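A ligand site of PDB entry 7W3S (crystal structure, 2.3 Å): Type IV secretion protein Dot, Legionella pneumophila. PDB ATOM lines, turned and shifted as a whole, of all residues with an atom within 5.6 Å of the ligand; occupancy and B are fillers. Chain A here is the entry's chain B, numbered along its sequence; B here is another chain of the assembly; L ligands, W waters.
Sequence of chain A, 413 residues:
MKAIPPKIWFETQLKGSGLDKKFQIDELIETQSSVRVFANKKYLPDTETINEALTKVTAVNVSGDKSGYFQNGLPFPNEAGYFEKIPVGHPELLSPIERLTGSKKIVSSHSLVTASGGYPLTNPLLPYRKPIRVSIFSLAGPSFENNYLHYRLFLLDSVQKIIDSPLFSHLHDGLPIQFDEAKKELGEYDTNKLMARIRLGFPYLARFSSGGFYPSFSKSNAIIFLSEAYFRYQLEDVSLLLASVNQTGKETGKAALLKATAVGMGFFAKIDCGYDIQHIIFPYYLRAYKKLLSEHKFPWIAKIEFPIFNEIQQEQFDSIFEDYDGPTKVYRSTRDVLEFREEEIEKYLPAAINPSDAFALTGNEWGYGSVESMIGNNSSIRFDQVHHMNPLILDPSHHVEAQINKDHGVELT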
ATOM      1  N   ASN A  61      21.202   7.809 -10.247  1.00  0.00           N
ATOM      2  CA  ASN A  61      22.139   7.094 -11.103  1.00  0.00           C
ATOM      3  C   ASN A  61      21.353   6.004 -11.830  1.00  0.00           C
ATOM      4  O   ASN A  61      20.845   5.071 -11.195  1.00  0.00           O
ATOM      5  CB  ASN A  61      23.267   6.517 -10.280  1.00  0.00           C
ATOM      6  CG  ASN A  61      24.435   6.026 -11.124  1.00  0.00           C
ATOM      7  OD1 ASN A  61      24.227   5.378 -12.141  1.00  0.00           O
ATOM      8  ND2 ASN A  61      25.648   6.307 -10.700  1.00  0.00           N
ATOM      9  N   VAL A  62      21.254   6.119 -13.155  1.00  0.00           N
ATOM     10  CA  VAL A  62      20.567   5.128 -13.979  1.00  0.00           C
ATOM     11  C   VAL A  62      21.431   4.803 -15.203  1.00  0.00           C
ATOM     12  O   VAL A  62      22.392   5.505 -15.517  1.00  0.00           O
ATOM     13  CB  VAL A  62      19.160   5.577 -14.412  1.00  0.00           C
ATOM     14  CG1 VAL A  62      18.219   5.600 -13.207  1.00  0.00           C
ATOM     15  CG2 VAL A  62      19.202   6.947 -15.074  1.00  0.00           C
ATOM     16  N   GLY A 117       1.819   0.409  -5.470  1.00  0.00           N
ATOM     17  CA  GLY A 117       1.659   0.514  -6.915  1.00  0.00           C
ATOM     18  C   GLY A 117       2.276   1.780  -7.485  1.00  0.00           C
ATOM     19  O   GLY A 117       2.931   2.573  -6.816  1.00  0.00           O
ATOM     20  N   TYR A 119       4.527   1.738 -10.167  1.00  0.00           N
ATOM     21  CA  TYR A 119       5.749   1.758 -10.968  1.00  0.00           C
ATOM     22  C   TYR A 119       5.483   1.118 -12.310  1.00  0.00           C
ATOM     23  O   TYR A 119       5.401   1.853 -13.306  1.00  0.00           O
ATOM     24  CB  TYR A 119       6.978   1.119 -10.337  1.00  0.00           C
ATOM     25  CG  TYR A 119       7.991   0.703 -11.394  1.00  0.00           C
ATOM     26  CD1 TYR A 119       8.415   1.588 -12.389  1.00  0.00           C
ATOM     27  CD2 TYR A 119       8.466  -0.606 -11.434  1.00  0.00           C
ATOM     28  CE1 TYR A 119       9.309   1.182 -13.370  1.00  0.00           C
ATOM     29  CE2 TYR A 119       9.360  -1.005 -12.403  1.00  0.00           C
ATOM     30  CZ  TYR A 119       9.782  -0.115 -13.360  1.00  0.00           C
ATOM     31  OH  TYR A 119      10.674  -0.553 -14.302  1.00  0.00           O
ATOM     32  N   PRO A 120       5.399  -0.216 -12.434  1.00  0.00           N
ATOM     33  CA  PRO A 120       5.249  -0.769 -13.781  1.00  0.00           C
ATOM     34  C   PRO A 120       4.013  -0.118 -14.371  1.00  0.00           C
ATOM     35  O   PRO A 120       3.043   0.169 -13.653  1.00  0.00           O
ATOM     36  CB  PRO A 120       5.071  -2.278 -13.552  1.00  0.00           C
ATOM     37  CG  PRO A 120       5.293  -2.504 -12.098  1.00  0.00           C
ATOM     38  CD  PRO A 120       5.004  -1.200 -11.408  1.00  0.00           C
ATOM     39  N   ASN A 123       0.475  -1.022 -13.353  1.00  0.00           N
ATOM     40  CA  ASN A 123       0.271  -1.269 -11.925  1.00  0.00           C
ATOM     41  C   ASN A 123      -0.129   0.037 -11.258  1.00  0.00           C
ATOM     42  O   ASN A 123       0.748   0.860 -10.938  1.00  0.00           O
ATOM     43  CB  ASN A 123       1.535  -1.872 -11.304  1.00  0.00           C
ATOM     44  CG  ASN A 123       1.399  -2.120  -9.831  1.00  0.00           C
ATOM     45  OD1 ASN A 123       0.289  -2.306  -9.322  1.00  0.00           O
ATOM     46  ND2 ASN A 123       2.519  -2.126  -9.126  1.00  0.00           N
ATOM     47  N   GLY A 141      21.423  -5.502  -5.570  1.00  0.00           N
ATOM     48  CA  GLY A 141      21.899  -6.742  -6.146  1.00  0.00           C
ATOM     49  C   GLY A 141      23.041  -6.516  -7.123  1.00  0.00           C
ATOM     50  O   GLY A 141      23.462  -5.385  -7.404  1.00  0.00           O
ATOM     51  N   GLU A 145      24.715  -3.700 -15.816  1.00  0.00           N
ATOM     52  CA  GLU A 145      24.391  -2.631 -16.771  1.00  0.00           C
ATOM     53  C   GLU A 145      25.619  -2.084 -17.489  1.00  0.00           C
ATOM     54  O   GLU A 145      25.507  -1.594 -18.618  1.00  0.00           O
ATOM     55  CB  GLU A 145      23.681  -1.471 -16.081  1.00  0.00           C
ATOM     56  CG  GLU A 145      22.275  -1.785 -15.619  1.00  0.00           C
ATOM     57  CD  GLU A 145      21.549  -0.540 -15.165  1.00  0.00           C
ATOM     58  OE1 GLU A 145      20.489  -0.231 -15.752  1.00  0.00           O
ATOM     59  OE2 GLU A 145      22.071   0.156 -14.242  1.00  0.00           O
ATOM     60  N   THR A 261      11.141  -9.324  -3.277  1.00  0.00           N
ATOM     61  CA  THR A 261      11.251  -8.694  -4.580  1.00  0.00           C
ATOM     62  C   THR A 261      12.410  -9.316  -5.346  1.00  0.00           C
ATOM     63  O   THR A 261      13.398  -9.775  -4.756  1.00  0.00           O
ATOM     64  CB  THR A 261      11.489  -7.184  -4.427  1.00  0.00           C
ATOM     65  OG1 THR A 261      10.694  -6.674  -3.358  1.00  0.00           O
ATOM     66  CG2 THR A 261      11.138  -6.419  -5.690  1.00  0.00           C
ATOM     67  N   ALA A 262      12.275  -9.331  -6.670  1.00  0.00           N
ATOM     68  CA  ALA A 262      13.278  -9.945  -7.537  1.00  0.00           C
ATOM     69  C   ALA A 262      14.427  -8.973  -7.830  1.00  0.00           C
ATOM     70  O   ALA A 262      14.665  -8.548  -8.959  1.00  0.00           O
ATOM     71  CB  ALA A 262      12.599 -10.419  -8.823  1.00  0.00           C
ATOM     72  N   VAL A 263      15.150  -8.617  -6.755  1.00  0.00           N
ATOM     73  CA  VAL A 263      16.352  -7.785  -6.785  1.00  0.00           C
ATOM     74  C   VAL A 263      17.248  -8.237  -7.917  1.00  0.00           C
ATOM     75  O   VAL A 263      17.483  -9.441  -8.072  1.00  0.00           O
ATOM     76  CB  VAL A 263      17.153  -7.891  -5.466  1.00  0.00           C
ATOM     77  CG1 VAL A 263      18.072  -6.705  -5.315  1.00  0.00           C
ATOM     78  CG2 VAL A 263      16.235  -8.127  -4.309  1.00  0.00           C
ATOM     79  N   GLY A 264      17.803  -7.291  -8.677  1.00  0.00           N
ATOM     80  CA  GLY A 264      18.762  -7.635  -9.713  1.00  0.00           C
ATOM     81  C   GLY A 264      18.160  -8.197 -10.989  1.00  0.00           C
ATOM     82  O   GLY A 264      18.904  -8.483 -11.946  1.00  0.00           O
ATOM     83  N   MET A 265      16.824  -8.306 -11.069  1.00  0.00           N
ATOM     84  CA  MET A 265      16.214  -9.028 -12.182  1.00  0.00           C
ATOM     85  C   MET A 265      15.552  -8.124 -13.230  1.00  0.00           C
ATOM     86  O   MET A 265      14.986  -8.612 -14.197  1.00  0.00           O
ATOM     87  CB  MET A 265      15.210 -10.031 -11.650  1.00  0.00           C
ATOM     88  CG  MET A 265      15.775 -10.942 -10.565  1.00  0.00           C
ATOM     89  SD  MET A 265      17.030 -12.159 -11.368  1.00  0.00           S
ATOM     90  CE  MET A 265      18.388 -12.215  -9.992  1.00  0.00           C
ATOM     91  N   GLY A 266      15.627  -6.809 -13.025  1.00  0.00           N
ATOM     92  CA  GLY A 266      15.075  -5.869 -13.983  1.00  0.00           C
ATOM     93  C   GLY A 266      16.186  -5.102 -14.671  1.00  0.00           C
ATOM     94  O   GLY A 266      16.929  -5.673 -15.474  1.00  0.00           O
ATOM     95  N   PHE A 267      16.311  -3.797 -14.345  1.00  0.00           N
ATOM     96  CA  PHE A 267      17.333  -2.960 -14.970  1.00  0.00           C
ATOM     97  C   PHE A 267      18.709  -3.594 -14.840  1.00  0.00           C
ATOM     98  O   PHE A 267      19.496  -3.591 -15.787  1.00  0.00           O
ATOM     99  CB  PHE A 267      17.345  -1.570 -14.337  1.00  0.00           C
ATOM    100  CG  PHE A 267      16.176  -0.712 -14.730  1.00  0.00           C
ATOM    101  CD1 PHE A 267      16.126  -0.117 -15.982  1.00  0.00           C
ATOM    102  CD2 PHE A 267      15.134  -0.492 -13.852  1.00  0.00           C
ATOM    103  CE1 PHE A 267      15.037   0.689 -16.359  1.00  0.00           C
ATOM    104  CE2 PHE A 267      14.029   0.309 -14.211  1.00  0.00           C
ATOM    105  CZ  PHE A 267      14.004   0.905 -15.464  1.00  0.00           C
ATOM    106  N   PHE A 268      18.997  -4.194 -13.678  1.00  0.00           N
ATOM    107  CA  PHE A 268      20.329  -4.705 -13.394  1.00  0.00           C
ATOM    108  C   PHE A 268      20.641  -6.011 -14.131  1.00  0.00           C
ATOM    109  O   PHE A 268      21.802  -6.418 -14.159  1.00  0.00           O
ATOM    110  CB  PHE A 268      20.491  -4.883 -11.875  1.00  0.00           C
ATOM    111  CG  PHE A 268      20.958  -3.640 -11.143  1.00  0.00           C
ATOM    112  CD1 PHE A 268      21.070  -2.428 -11.809  1.00  0.00           C
ATOM    113  CD2 PHE A 268      21.288  -3.694  -9.798  1.00  0.00           C
ATOM    114  CE1 PHE A 268      21.513  -1.282 -11.155  1.00  0.00           C
ATOM    115  CE2 PHE A 268      21.736  -2.560  -9.116  1.00  0.00           C
ATOM    116  CZ  PHE A 268      21.852  -1.347  -9.806  1.00  0.00           C
ATOM    117  N   ALA A 269      19.649  -6.667 -14.732  1.00  0.00           N
ATOM    118  CA  ALA A 269      19.898  -7.913 -15.457  1.00  0.00           C
ATOM    119  C   ALA A 269      20.177  -7.680 -16.950  1.00  0.00           C
ATOM    120  O   ALA A 269      20.203  -8.647 -17.725  1.00  0.00           O
ATOM    121  CB  ALA A 269      18.710  -8.862 -15.299  1.00  0.00           C
ATOM    122  N   PRO A 307       6.915 -11.805  -5.596  1.00  0.00           N
ATOM    123  CA  PRO A 307       6.152 -11.243  -6.704  1.00  0.00           C
ATOM    124  C   PRO A 307       6.853 -11.559  -8.014  1.00  0.00           C
ATOM    125  O   PRO A 307       8.014 -11.201  -8.223  1.00  0.00           O
ATOM    126  CB  PRO A 307       6.138  -9.736  -6.410  1.00  0.00           C
ATOM    127  CG  PRO A 307       6.844  -9.558  -5.091  1.00  0.00           C
ATOM    128  CD  PRO A 307       7.682 -10.782  -4.875  1.00  0.00           C
ATOM    129  N   PHE A 309       5.983 -11.820 -12.208  1.00  0.00           N
ATOM    130  CA  PHE A 309       5.018 -11.447 -13.220  1.00  0.00           C
ATOM    131  C   PHE A 309       5.270 -12.094 -14.579  1.00  0.00           C
ATOM    132  O   PHE A 309       4.351 -12.125 -15.397  1.00  0.00           O
ATOM    133  CB  PHE A 309       5.015  -9.926 -13.365  1.00  0.00           C
ATOM    134  CG  PHE A 309       4.828  -9.219 -12.060  1.00  0.00           C
ATOM    135  CD1 PHE A 309       3.574  -9.159 -11.477  1.00  0.00           C
ATOM    136  CD2 PHE A 309       5.908  -8.674 -11.392  1.00  0.00           C
ATOM    137  CE1 PHE A 309       3.394  -8.548 -10.267  1.00  0.00           C
ATOM    138  CE2 PHE A 309       5.720  -8.041 -10.161  1.00  0.00           C
ATOM    139  CZ  PHE A 309       4.474  -7.981  -9.594  1.00  0.00           C
ATOM    140  N   GLN A 313       9.647 -17.004 -15.523  1.00  0.00           N
ATOM    141  CA  GLN A 313      10.028 -16.901 -14.122  1.00  0.00           C
ATOM    142  C   GLN A 313       9.085 -17.701 -13.242  1.00  0.00           C
ATOM    143  O   GLN A 313       9.522 -18.491 -12.385  1.00  0.00           O
ATOM    144  CB  GLN A 313      10.029 -15.439 -13.697  1.00  0.00           C
ATOM    145  CG  GLN A 313      11.078 -14.578 -14.342  1.00  0.00           C
ATOM    146  CD  GLN A 313      11.041 -13.160 -13.791  1.00  0.00           C
ATOM    147  OE1 GLN A 313      10.018 -12.473 -13.862  1.00  0.00           O
ATOM    148  NE2 GLN A 313      12.165 -12.714 -13.226  1.00  0.00           N
ATOM    149  N   ARG A 335       1.192  -9.724  -6.694  1.00  0.00           N
ATOM    150  CA  ARG A 335       0.822  -8.570  -5.882  1.00  0.00           C
ATOM    151  C   ARG A 335       2.009  -7.608  -5.771  1.00  0.00           C
ATOM    152  O   ARG A 335       3.156  -8.037  -5.671  1.00  0.00           O
ATOM    153  CB  ARG A 335       0.342  -9.032  -4.509  1.00  0.00           C
ATOM    154  CG  ARG A 335       0.142  -7.922  -3.485  1.00  0.00           C
ATOM    155  CD  ARG A 335      -0.706  -8.405  -2.328  1.00  0.00           C
ATOM    156  NE  ARG A 335       0.010  -9.365  -1.483  1.00  0.00           N
ATOM    157  CZ  ARG A 335      -0.382  -9.698  -0.252  1.00  0.00           C
ATOM    158  NH1 ARG A 335      -1.487  -9.157   0.260  1.00  0.00           N
ATOM    159  NH2 ARG A 335       0.321 -10.562   0.461  1.00  0.00           N
ATOM    160  N   ASP A 336       1.718  -6.303  -5.828  1.00  0.00           N
ATOM    161  CA  ASP A 336       2.732  -5.269  -5.668  1.00  0.00           C
ATOM    162  C   ASP A 336       3.506  -5.411  -4.355  1.00  0.00           C
ATOM    163  O   ASP A 336       2.941  -5.841  -3.333  1.00  0.00           O
ATOM    164  CB  ASP A 336       2.055  -3.897  -5.716  1.00  0.00           C
ATOM    165  CG  ASP A 336       3.026  -2.750  -5.531  1.00  0.00           C
ATOM    166  OD1 ASP A 336       3.574  -2.300  -6.563  1.00  0.00           O
ATOM    167  OD2 ASP A 336       3.246  -2.287  -4.378  1.00  0.00           O
ATOM    168  N   VAL A 337       4.788  -5.021  -4.378  1.00  0.00           N
ATOM    169  CA  VAL A 337       5.672  -5.084  -3.207  1.00  0.00           C
ATOM    170  C   VAL A 337       5.011  -4.576  -1.944  1.00  0.00           C
ATOM    171  O   VAL A 337       5.068  -5.228  -0.893  1.00  0.00           O
ATOM    172  CB  VAL A 337       6.959  -4.251  -3.350  1.00  0.00           C
ATOM    173  CG1 VAL A 337       8.143  -5.103  -3.079  1.00  0.00           C
ATOM    174  CG2 VAL A 337       7.028  -3.452  -4.617  1.00  0.00           C
ATOM    175  N   PRO A 355      14.897  -3.223  -4.034  1.00  0.00           N
ATOM    176  CA  PRO A 355      16.067  -3.532  -4.872  1.00  0.00           C
ATOM    177  C   PRO A 355      16.799  -2.250  -5.233  1.00  0.00           C
ATOM    178  O   PRO A 355      16.370  -1.476  -6.098  1.00  0.00           O
ATOM    179  CB  PRO A 355      15.447  -4.226  -6.100  1.00  0.00           C
ATOM    180  CG  PRO A 355      14.085  -3.680  -6.188  1.00  0.00           C
ATOM    181  CD  PRO A 355      13.633  -3.359  -4.777  1.00  0.00           C
ATOM    182  N   SER A 356      17.886  -2.011  -4.535  1.00  0.00           N
ATOM    183  CA  SER A 356      18.447  -0.679  -4.429  1.00  0.00           C
ATOM    184  C   SER A 356      19.655  -0.521  -5.352  1.00  0.00           C
ATOM    185  O   SER A 356      19.939  -1.368  -6.199  1.00  0.00           O
ATOM    186  CB  SER A 356      18.776  -0.407  -2.951  1.00  0.00           C
ATOM    187  OG  SER A 356      18.971   0.986  -2.756  1.00  0.00           O
ATOM    188  N   ASP A 357      20.351   0.601  -5.204  1.00  0.00           N
ATOM    189  CA  ASP A 357      21.557   0.922  -5.961  1.00  0.00           C
ATOM    190  C   ASP A 357      22.683   1.221  -4.971  1.00  0.00           C
ATOM    191  O   ASP A 357      22.509   2.033  -4.063  1.00  0.00           O
ATOM    192  CB  ASP A 357      21.336   2.149  -6.854  1.00  0.00           C
ATOM    193  CG  ASP A 357      22.458   2.320  -7.890  1.00  0.00           C
ATOM    194  OD1 ASP A 357      23.625   2.594  -7.502  1.00  0.00           O
ATOM    195  OD2 ASP A 357      22.148   2.158  -9.100  1.00  0.00           O
ATOM    196  N   GLY A 363      16.213   5.571  -2.669  1.00  0.00           N
ATOM    197  CA  GLY A 363      15.144   6.192  -3.421  1.00  0.00           C
ATOM    198  C   GLY A 363      15.536   6.369  -4.882  1.00  0.00           C
ATOM    199  O   GLY A 363      14.749   6.067  -5.785  1.00  0.00           O
ATOM    200  N   ASN A 364      16.762   6.838  -5.123  1.00  0.00           N
ATOM    201  CA  ASN A 364      17.343   7.021  -6.474  1.00  0.00           C
ATOM    202  C   ASN A 364      16.469   8.003  -7.255  1.00  0.00           C
ATOM    203  O   ASN A 364      16.262   9.134  -6.775  1.00  0.00           O
ATOM    204  CB  ASN A 364      17.521   5.662  -7.118  1.00  0.00           C
ATOM    205  CG  ASN A 364      18.534   5.677  -8.226  1.00  0.00           C
ATOM    206  OD1 ASN A 364      18.971   6.737  -8.670  1.00  0.00           O
ATOM    207  ND2 ASN A 364      18.893   4.483  -8.720  1.00  0.00           N
ATOM    208  N   GLU A 365      15.981   7.667  -8.448  1.00  0.00           N
ATOM    209  CA  GLU A 365      15.210   8.589  -9.273  1.00  0.00           C
ATOM    210  C   GLU A 365      13.994   9.093  -8.505  1.00  0.00           C
ATOM    211  O   GLU A 365      13.510   8.443  -7.575  1.00  0.00           O
ATOM    212  CB  GLU A 365      14.714   7.925 -10.559  1.00  0.00           C
ATOM    213  CG  GLU A 365      15.756   7.402 -11.494  1.00  0.00           C
ATOM    214  CD  GLU A 365      15.131   6.738 -12.714  1.00  0.00           C
ATOM    215  OE1 GLU A 365      14.415   5.706 -12.567  1.00  0.00           O
ATOM    216  OE2 GLU A 365      15.359   7.254 -13.839  1.00  0.00           O
ATOM    217  N   SER A 370      11.170   2.938 -11.404  1.00  0.00           N
ATOM    218  CA  SER A 370      11.782   1.682 -10.963  1.00  0.00           C
ATOM    219  C   SER A 370      11.088   1.236  -9.694  1.00  0.00           C
ATOM    220  O   SER A 370      10.348   2.005  -9.065  1.00  0.00           O
ATOM    221  CB  SER A 370      13.275   1.864 -10.695  1.00  0.00           C
ATOM    222  OG  SER A 370      13.436   2.761  -9.608  1.00  0.00           O
ATOM    223  N   VAL A 371      11.354   0.002  -9.286  1.00  0.00           N
ATOM    224  CA  VAL A 371      10.800  -0.438  -8.008  1.00  0.00           C
ATOM    225  C   VAL A 371      11.281   0.472  -6.888  1.00  0.00           C
ATOM    226  O   VAL A 371      10.484   0.961  -6.076  1.00  0.00           O
ATOM    227  CB  VAL A 371      11.126  -1.918  -7.734  1.00  0.00           C
ATOM    228  CG1 VAL A 371      10.631  -2.269  -6.328  1.00  0.00           C
ATOM    229  CG2 VAL A 371      10.470  -2.830  -8.810  1.00  0.00           C
ATOM    230  N   GLU A 372      12.597   0.767  -6.859  1.00  0.00           N
ATOM    231  CA  GLU A 372      13.131   1.609  -5.794  1.00  0.00           C
ATOM    232  C   GLU A 372      12.512   3.012  -5.796  1.00  0.00           C
ATOM    233  O   GLU A 372      12.092   3.519  -4.750  1.00  0.00           O
ATOM    234  CB  GLU A 372      14.652   1.727  -5.889  1.00  0.00           C
ATOM    235  CG  GLU A 372      15.180   2.849  -4.974  1.00  0.00           C
ATOM    236  CD  GLU A 372      16.590   2.620  -4.459  1.00  0.00           C
ATOM    237  OE1 GLU A 372      17.531   2.543  -5.309  1.00  0.00           O
ATOM    238  OE2 GLU A 372      16.753   2.554  -3.214  1.00  0.00           O
ATOM    239  N   MET A 374       9.699   3.951  -7.042  1.00  0.00           N
ATOM    240  CA  MET A 374       8.312   3.802  -6.599  1.00  0.00           C
ATOM    241  C   MET A 374       8.180   3.739  -5.074  1.00  0.00           C
ATOM    242  O   MET A 374       7.378   4.470  -4.480  1.00  0.00           O
ATOM    243  CB  MET A 374       7.677   2.551  -7.142  1.00  0.00           C
ATOM    244  CG  MET A 374       6.363   2.249  -6.438  1.00  0.00           C
ATOM    245  SD  MET A 374       5.588   0.616  -7.123  1.00  0.00           S
ATOM    246  CE  MET A 374       6.995  -0.579  -6.574  1.00  0.00           C
ATOM    247  N   LYS B  21      10.244  -1.768 -20.529  1.00  0.00           N
ATOM    248  CA  LYS B  21      11.201  -1.482 -19.466  1.00  0.00           C
ATOM    249  C   LYS B  21      11.847  -0.111 -19.648  1.00  0.00           C
ATOM    250  O   LYS B  21      12.093   0.595 -18.659  1.00  0.00           O
ATOM    251  CB  LYS B  21      12.271  -2.564 -19.394  1.00  0.00           C
ATOM    252  CG  LYS B  21      13.132  -2.558 -18.115  1.00  0.00           C
ATOM    253  CD  LYS B  21      12.274  -2.588 -16.815  1.00  0.00           C
ATOM    254  CE  LYS B  21      13.127  -2.835 -15.555  1.00  0.00           C
ATOM    255  NZ  LYS B  21      12.434  -2.610 -14.225  1.00  0.00           N
HETATM  256  N1  LIG L   1       6.225  -5.128  -7.228  1.00  0.00           N
HETATM  257  C1  LIG L   1       7.059  -6.183  -7.085  1.00  0.00           C
HETATM  258  N2  LIG L   1       7.986  -6.453  -8.030  1.00  0.00           N
HETATM  259  C2  LIG L   1       8.067  -5.673  -9.123  1.00  0.00           C
HETATM  260  C3  LIG L   1       7.249  -4.623  -9.264  1.00  0.00           C
HETATM  261  C4  LIG L   1       6.339  -4.345  -8.292  1.00  0.00           C
HETATM  262  N3  LIG L   1       5.395  -3.271  -8.315  1.00  0.00           N
HETATM  263  N4  LIG L   1       7.520  -3.984 -10.418  1.00  0.00           N
HETATM  264  C5  LIG L   1       8.518  -4.620 -11.024  1.00  0.00           C
HETATM  265  N5  LIG L   1       8.822  -5.626 -10.216  1.00  0.00           N
HETATM  266  P1  LIG L   1      14.021  -3.221 -10.774  1.00  0.00           P
HETATM  267  P2  LIG L   1      16.905  -3.973 -10.349  1.00  0.00           P
HETATM  268  C6  LIG L   1       9.739  -6.730 -10.186  1.00  0.00           C
HETATM  269  O1  LIG L   1      14.175  -3.394 -12.272  1.00  0.00           O
HETATM  270  O2  LIG L   1      17.018  -4.968 -11.497  1.00  0.00           O
HETATM  271  C7  LIG L   1      16.742   1.256  -9.780  1.00  0.00           C
HETATM  272  O3  LIG L   1      17.116   2.462 -10.434  1.00  0.00           O
HETATM  273  C8  LIG L   1      10.169  -6.941 -11.445  1.00  0.00           C
HETATM  274  O4  LIG L   1      10.388  -8.335 -11.728  1.00  0.00           O
HETATM  275  O5  LIG L   1      13.454  -1.868 -10.446  1.00  0.00           O
HETATM  276  O6  LIG L   1      17.397  -4.661  -9.072  1.00  0.00           O
HETATM  277  C9  LIG L   1      17.697   0.942  -8.577  1.00  0.00           C
HETATM  278  O7  LIG L   1      17.954   2.017  -7.798  1.00  0.00           O
HETATM  279  C10 LIG L   1      11.607  -6.181 -11.556  1.00  0.00           C
HETATM  280  O8  LIG L   1      12.316  -6.725 -12.646  1.00  0.00           O
HETATM  281  O9  LIG L   1      15.414  -3.413  -9.954  1.00  0.00           O
HETATM  282  C11 LIG L   1      18.904   0.476  -9.332  1.00  0.00           C
HETATM  283  O10 LIG L   1      19.540   1.624 -10.042  1.00  0.00           O
HETATM  284  C12 LIG L   1      12.182  -6.550 -10.387  1.00  0.00           C
HETATM  285  O11 LIG L   1      11.037  -6.306  -9.393  1.00  0.00           O
HETATM  286  C13 LIG L   1      18.359  -0.362 -10.241  1.00  0.00           C
HETATM  287  O12 LIG L   1      16.922   0.243 -10.600  1.00  0.00           O
HETATM  288  C14 LIG L   1      13.400  -5.679 -10.084  1.00  0.00           C
HETATM  289  O13 LIG L   1      12.986  -4.343 -10.207  1.00  0.00           O
HETATM  290  C15 LIG L   1      18.179  -1.746  -9.672  1.00  0.00           C
HETATM  291  O14 LIG L   1      17.764  -2.607 -10.723  1.00  0.00           O
HETATM  292  O   HOH W   1       9.536  -8.918  -7.524  1.00  0.00           O
HETATM  293  O   HOH W   2      19.072  -4.072  -6.806  1.00  0.00           O
HETATM  294  O   HOH W   3      15.755   4.732  -9.979  1.00  0.00           O
HETATM  295  O   HOH W   4      12.069  -9.649 -13.578  1.00  0.00           O
HETATM  296  O   HOH W   5      14.517  -0.584  -8.187  1.00  0.00           O
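The backbone NH of Asp 357 sits at hydrogen-bond distance from the side-chain carboxylate of Glu 372 (3.4 Å). The side-chain hydroxyl (OG) of Ser 370 lies close to the backbone NH (N) of Glu 372 (3.5 Å). The side-chain carboxylate of Glu 372 is in hydrogen-bond range of the side-chain hydroxyl of Ser 356 (2.8 Å). OE2 of Glu 372 is in hydrogen-bond range of N of Gly 363, 3.1 Å away. The backbone carbonyl oxygen (O) of Gly 264 lies close to the backbone NH (N) of Ala 269, 3.4 Å away. OD1 of Asp 336 is in hydrogen-bond range of ND2 of Asn 123, at 2.8 Å. OD2 of Asp 336 lies within hydrogen-bond range of N of Gly 117 (3.2 Å). The side-chain amide oxygen of Asn 364 is in hydrogen-bond range of the backbone NH of Asn 61.
Asn 61 touches the ligand (O to O10, 3.9 Å). Tyr 119 touches the ligand (CD2 to N4, 3.7 Å). Pro 120 touches the ligand (CG to N4, 3.2 Å). CG2 of Thr 261 touches O11 of the ligand, 3.7 Å away. O of Ala 262 touches C14 of the ligand (3.3 Å). Val 263 touches the ligand. Pro 307 touches the ligand (CB to C1, 3.7 Å). Phe 309 touches the ligand (CE2 to C2, 3.5 Å). Pro 355 touches the ligand. O of Ser 356 touches C11 of the ligand (3.8 Å). OG of Ser 370 touches C7 of the ligand, at 3.6 Å. CE of Met 374 touches N3 of the ligand (3.6 Å). The nearest printed residue that does not touch the ligand is Val 62 (4.3 Å).
The side-chain carboxylate (OE1) of Glu 372 lies within hydrogen-bond range of an oxygen (O7) of the ligand, 2.6 Å away. O6 of the ligand lies within hydrogen-bond range of N of Gly 264. OD1 of Asp 336 lies within hydrogen-bond range of N3 of the ligand. The side-chain amino group (NZ) of Lys 21 of chain B is in salt-bridge range of an oxygen (O1) of the ligand (2.7 Å). N of Gly 266 sits at hydrogen-bond distance from O2 of the ligand, 2.8 Å away. O7 of the ligand sits at hydrogen-bond distance from ND2 of Asn 364 (2.8 Å). An oxygen (O10) of the ligand lies within hydrogen-bond range of the side-chain carboxylate (OD2) of Asp 357 (2.8 Å). N of Phe 267 sits at hydrogen-bond distance from O1 of the ligand. An oxygen (O5) of the ligand is in hydrogen-bond range of the backbone NH of Val 371, 3.0 Å away. An oxygen (O2) of the ligand is in hydrogen-bond range of the backbone NH (N) of Phe 268, at 3.0 Å. N of Val 337 is in hydrogen-bond range of N1 of the ligand, 3.2 Å away. The side-chain amide nitrogen (ND2) of Asn 123 sits close to a nitrogen (N3) of the ligand, 3.2 Å away. The backbone NH (N) of Met 265 is in hydrogen-bond range of an oxygen (O2) of the ligand.
Water W3 lies within hydrogen-bond range of an oxygen (O3) of the ligand, the side-chain hydroxyl of Ser 370, the side-chain carboxylate of Glu 365 and the side-chain amide nitrogen of Asn 364. Water W5 lies within hydrogen-bond range of N of Glu 372 (2.7 Å), O5 of the ligand (2.8 Å), O of Pro 355 (2.9 Å) and N of Val 371 (3.4 Å). Water W4 lies within hydrogen-bond range of O4 of the ligand, NE2 of Gln 313 and O of Met 265. Water W2 lies within hydrogen-bond range of O6 of the ligand (2.9 Å), O of Ser 356 (2.9 Å) and N of Gly 141 (3.0 Å). Water W1 lies within hydrogen-bond range of O of Pro 307 (2.8 Å), N of Ala 262 (2.9 Å) and N2 of the ligand (3.0 Å).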
